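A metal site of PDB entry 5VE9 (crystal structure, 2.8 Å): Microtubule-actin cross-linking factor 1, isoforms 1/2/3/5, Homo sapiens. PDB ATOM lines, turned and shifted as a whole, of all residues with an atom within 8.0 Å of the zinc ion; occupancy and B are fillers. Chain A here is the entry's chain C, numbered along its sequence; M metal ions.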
ATOM      1  N   VAL A  13      16.500 -20.650   5.793  1.00  0.00           N
ATOM      2  CA  VAL A  13      17.464 -21.275   4.887  1.00  0.00           C
ATOM      3  C   VAL A  13      17.325 -20.666   3.501  1.00  0.00           C
ATOM      4  O   VAL A  13      18.243 -20.767   2.673  1.00  0.00           O
ATOM      5  CB  VAL A  13      17.265 -22.809   4.822  1.00  0.00           C
ATOM      6  CG1 VAL A  13      18.221 -23.443   3.811  1.00  0.00           C
ATOM      7  CG2 VAL A  13      17.491 -23.422   6.194  1.00  0.00           C
ATOM      8  N   GLN A  15      17.445 -17.648   2.982  1.00  0.00           N
ATOM      9  CA  GLN A  15      18.357 -16.519   3.015  1.00  0.00           C
ATOM     10  C   GLN A  15      19.751 -16.860   2.476  1.00  0.00           C
ATOM     11  O   GLN A  15      20.620 -15.990   2.407  1.00  0.00           O
ATOM     12  CB  GLN A  15      18.492 -15.987   4.448  1.00  0.00           C
ATOM     13  CG  GLN A  15      17.188 -15.549   5.083  1.00  0.00           C
ATOM     14  CD  GLN A  15      17.326 -15.295   6.571  1.00  0.00           C
ATOM     15  OE1 GLN A  15      18.384 -15.524   7.163  1.00  0.00           O
ATOM     16  NE2 GLN A  15      16.246 -14.815   7.188  1.00  0.00           N
ATOM     17  N   CYS A  16      19.959 -18.122   2.100  1.00  0.00           N
ATOM     18  CA  CYS A  16      21.270 -18.557   1.623  1.00  0.00           C
ATOM     19  C   CYS A  16      21.614 -17.896   0.287  1.00  0.00           C
ATOM     20  O   CYS A  16      20.785 -17.832  -0.621  1.00  0.00           O
ATOM     21  CB  CYS A  16      21.311 -20.077   1.469  1.00  0.00           C
ATOM     22  SG  CYS A  16      22.943 -20.708   1.013  1.00  0.00           S
ATOM     23  N   LYS A  17      22.857 -17.415   0.183  1.00  0.00           N
ATOM     24  CA  LYS A  17      23.328 -16.725  -1.013  1.00  0.00           C
ATOM     25  C   LYS A  17      24.343 -17.557  -1.795  1.00  0.00           C
ATOM     26  O   LYS A  17      24.983 -17.060  -2.724  1.00  0.00           O
ATOM     27  CB  LYS A  17      23.944 -15.379  -0.632  1.00  0.00           C
ATOM     28  CG  LYS A  17      22.934 -14.267  -0.420  1.00  0.00           C
ATOM     29  CD  LYS A  17      23.540 -13.077   0.326  1.00  0.00           C
ATOM     30  CE  LYS A  17      24.829 -12.594  -0.329  1.00  0.00           C
ATOM     31  NZ  LYS A  17      25.365 -11.367   0.332  1.00  0.00           N
ATOM     32  N   CYS A  18      24.503 -18.822  -1.422  1.00  0.00           N
ATOM     33  CA  CYS A  18      25.455 -19.704  -2.091  1.00  0.00           C
ATOM     34  C   CYS A  18      24.961 -20.067  -3.498  1.00  0.00           C
ATOM     35  O   CYS A  18      23.768 -19.995  -3.787  1.00  0.00           O
ATOM     36  CB  CYS A  18      25.678 -20.985  -1.275  1.00  0.00           C
ATOM     37  SG  CYS A  18      26.300 -20.730   0.402  1.00  0.00           S
ATOM     38  N   ALA A  19      25.904 -20.441  -4.362  1.00  0.00           N
ATOM     39  CA  ALA A  19      25.552 -20.977  -5.669  1.00  0.00           C
ATOM     40  C   ALA A  19      24.794 -22.282  -5.456  1.00  0.00           C
ATOM     41  O   ALA A  19      23.676 -22.457  -5.941  1.00  0.00           O
ATOM     42  CB  ALA A  19      26.791 -21.198  -6.519  1.00  0.00           C
ATOM     43  N   LYS A  20      25.433 -23.202  -4.743  1.00  0.00           N
ATOM     44  CA  LYS A  20      24.753 -24.373  -4.209  1.00  0.00           C
ATOM     45  C   LYS A  20      24.089 -23.975  -2.897  1.00  0.00           C
ATOM     46  O   LYS A  20      24.698 -24.054  -1.835  1.00  0.00           O
ATOM     47  CB  LYS A  20      25.720 -25.530  -3.979  1.00  0.00           C
ATOM     48  CG  LYS A  20      25.938 -26.432  -5.184  1.00  0.00           C
ATOM     49  CD  LYS A  20      27.045 -27.441  -4.921  1.00  0.00           C
ATOM     50  CE  LYS A  20      26.837 -28.728  -5.695  1.00  0.00           C
ATOM     51  NZ  LYS A  20      27.886 -29.731  -5.375  1.00  0.00           N
ATOM     52  N   ARG A  21      22.845 -23.529  -2.993  1.00  0.00           N
ATOM     53  CA  ARG A  21      22.139 -22.993  -1.834  1.00  0.00           C
ATOM     54  C   ARG A  21      22.056 -24.016  -0.718  1.00  0.00           C
ATOM     55  O   ARG A  21      21.768 -25.191  -0.941  1.00  0.00           O
ATOM     56  CB  ARG A  21      20.745 -22.519  -2.245  1.00  0.00           C
ATOM     57  CG  ARG A  21      20.780 -21.401  -3.275  1.00  0.00           C
ATOM     58  CD  ARG A  21      19.390 -21.044  -3.787  1.00  0.00           C
ATOM     59  NE  ARG A  21      18.561 -20.415  -2.766  1.00  0.00           N
ATOM     60  CZ  ARG A  21      17.759 -21.083  -1.927  1.00  0.00           C
ATOM     61  NH1 ARG A  21      17.671 -22.403  -1.975  1.00  0.00           N
ATOM     62  NH2 ARG A  21      17.048 -20.409  -1.031  1.00  0.00           N
ATOM     63  N   PHE A  22      22.354 -23.541   0.498  1.00  0.00           N
ATOM     64  CA  PHE A  22      22.405 -24.372   1.699  1.00  0.00           C
ATOM     65  C   PHE A  22      21.243 -25.360   1.763  1.00  0.00           C
ATOM     66  O   PHE A  22      20.080 -24.960   1.711  1.00  0.00           O
ATOM     67  CB  PHE A  22      22.403 -23.494   2.954  1.00  0.00           C
ATOM     68  CG  PHE A  22      22.834 -24.224   4.201  1.00  0.00           C
ATOM     69  CD1 PHE A  22      24.167 -24.519   4.416  1.00  0.00           C
ATOM     70  CD2 PHE A  22      21.906 -24.602   5.164  1.00  0.00           C
ATOM     71  CE1 PHE A  22      24.564 -25.189   5.564  1.00  0.00           C
ATOM     72  CE2 PHE A  22      22.307 -25.263   6.302  1.00  0.00           C
ATOM     73  CZ  PHE A  22      23.632 -25.557   6.505  1.00  0.00           C
ATOM     74  N   GLN A  23      21.566 -26.637   1.889  1.00  0.00           N
ATOM     75  CA  GLN A  23      20.548 -27.680   1.834  1.00  0.00           C
ATOM     76  C   GLN A  23      20.208 -28.204   3.217  1.00  0.00           C
ATOM     77  O   GLN A  23      21.083 -28.403   4.063  1.00  0.00           O
ATOM     78  CB  GLN A  23      21.000 -28.834   0.933  1.00  0.00           C
ATOM     79  CG  GLN A  23      22.357 -29.398   1.256  1.00  0.00           C
ATOM     80  CD  GLN A  23      22.626 -30.685   0.496  1.00  0.00           C
ATOM     81  OE1 GLN A  23      23.565 -31.419   0.816  1.00  0.00           O
ATOM     82  NE2 GLN A  23      21.808 -30.972  -0.516  1.00  0.00           N
ATOM     83  N   LEU A  65      22.877 -21.276  11.721  1.00  0.00           N
ATOM     84  CA  LEU A  65      23.119 -21.040  10.297  1.00  0.00           C
ATOM     85  C   LEU A  65      24.315 -20.114  10.093  1.00  0.00           C
ATOM     86  O   LEU A  65      25.134 -20.331   9.208  1.00  0.00           O
ATOM     87  CB  LEU A  65      21.882 -20.442   9.632  1.00  0.00           C
ATOM     88  CG  LEU A  65      20.650 -21.344   9.564  1.00  0.00           C
ATOM     89  CD1 LEU A  65      19.444 -20.570   9.043  1.00  0.00           C
ATOM     90  CD2 LEU A  65      20.922 -22.561   8.690  1.00  0.00           C
ATOM     91  N   ASN A  68      27.215 -22.325  10.356  1.00  0.00           N
ATOM     92  CA  ASN A  68      27.328 -23.477   9.450  1.00  0.00           C
ATOM     93  C   ASN A  68      27.052 -23.166   7.977  1.00  0.00           C
ATOM     94  O   ASN A  68      27.485 -23.904   7.107  1.00  0.00           O
ATOM     95  CB  ASN A  68      26.383 -24.580   9.919  1.00  0.00           C
ATOM     96  CG  ASN A  68      26.833 -25.223  11.206  1.00  0.00           C
ATOM     97  OD1 ASN A  68      26.498 -24.772  12.296  1.00  0.00           O
ATOM     98  ND2 ASN A  68      27.622 -26.285  11.088  1.00  0.00           N
ATOM     99  N   ASP A  69      26.323 -22.085   7.699  1.00  0.00           N
ATOM    100  CA  ASP A  69      26.063 -21.664   6.322  1.00  0.00           C
ATOM    101  C   ASP A  69      27.163 -20.676   5.890  1.00  0.00           C
ATOM    102  O   ASP A  69      27.318 -19.622   6.513  1.00  0.00           O
ATOM    103  CB  ASP A  69      24.678 -21.032   6.203  1.00  0.00           C
ATOM    104  CG  ASP A  69      24.303 -20.713   4.764  1.00  0.00           C
ATOM    105  OD1 ASP A  69      24.956 -21.241   3.837  1.00  0.00           O
ATOM    106  OD2 ASP A  69      23.352 -19.936   4.560  1.00  0.00           O
ATOM    107  N   PRO A  70      27.932 -21.017   4.838  1.00  0.00           N
ATOM    108  CA  PRO A  70      29.115 -20.182   4.565  1.00  0.00           C
ATOM    109  C   PRO A  70      28.801 -18.764   4.088  1.00  0.00           C
ATOM    110  O   PRO A  70      29.598 -17.855   4.336  1.00  0.00           O
ATOM    111  CB  PRO A  70      29.838 -20.951   3.455  1.00  0.00           C
ATOM    112  CG  PRO A  70      29.243 -22.314   3.450  1.00  0.00           C
ATOM    113  CD  PRO A  70      27.833 -22.141   3.905  1.00  0.00           C
ATOM    114  N   CYS A  71      27.668 -18.562   3.415  1.00  0.00           N
ATOM    115  CA  CYS A  71      27.320 -17.248   2.908  1.00  0.00           C
ATOM    116  C   CYS A  71      27.034 -16.244   4.024  1.00  0.00           C
ATOM    117  O   CYS A  71      26.815 -15.064   3.767  1.00  0.00           O
ATOM    118  CB  CYS A  71      26.113 -17.336   1.971  1.00  0.00           C
ATOM    119  SG  CYS A  71      24.564 -17.756   2.788  1.00  0.00           S
ATOM    120  N   ARG A  72      27.038 -16.726   5.276  1.00  0.00           N
ATOM    121  CA  ARG A  72      26.888 -15.846   6.434  1.00  0.00           C
ATOM    122  C   ARG A  72      28.064 -15.988   7.383  1.00  0.00           C
ATOM    123  O   ARG A  72      28.171 -15.231   8.348  1.00  0.00           O
ATOM    124  CB  ARG A  72      25.593 -16.156   7.196  1.00  0.00           C
ATOM    125  CG  ARG A  72      24.446 -16.682   6.360  1.00  0.00           C
ATOM    126  CD  ARG A  72      23.418 -17.379   7.236  1.00  0.00           C
ATOM    127  NE  ARG A  72      22.658 -18.365   6.486  1.00  0.00           N
ATOM    128  CZ  ARG A  72      21.335 -18.392   6.350  1.00  0.00           C
ATOM    129  NH1 ARG A  72      20.570 -17.475   6.924  1.00  0.00           N
ATOM    130  NH2 ARG A  72      20.774 -19.357   5.632  1.00  0.00           N
ATOM    131  N   ALA A  73      28.934 -16.970   7.142  1.00  0.00           N
ATOM    132  CA  ALA A  73      30.041 -17.251   8.055  1.00  0.00           C
ATOM    133  C   ALA A  73      31.202 -16.270   7.863  1.00  0.00           C
ATOM    134  O   ALA A  73      32.349 -16.686   7.686  1.00  0.00           O
ATOM    135  CB  ALA A  73      30.510 -18.682   7.872  1.00  0.00           C
HETATM  136 ZN    ZN M   1      24.901 -20.080   2.129  1.00  0.00          ZN
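The zinc ion is bound by the side-chain carboxylate (OD1) of Asp 69 (2.1 Å), the side-chain sulfur (SG) of Cys 18 (2.3 Å), the side-chain sulfur (SG) of Cys 16 (2.3 Å) and the side-chain sulfur (SG) of Cys 71 (2.4 Å).
NE of Arg 72 is in salt-bridge range of OD2 of Asp 69 (2.6 Å).
SG of Cys 16 lies close to N of Phe 22 (2.9 Å).
The side-chain sulfur (SG) of Cys 71 lies close to the backbone NH (N) of Lys 17, at 3.1 Å.
Residues that only touch the zinc ion: Lys 17 and Pro 70.
Within 4 Å of the zinc ion: Cys 16, Lys 17, Cys 18, Asp 69, Pro 70 and Cys 71.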
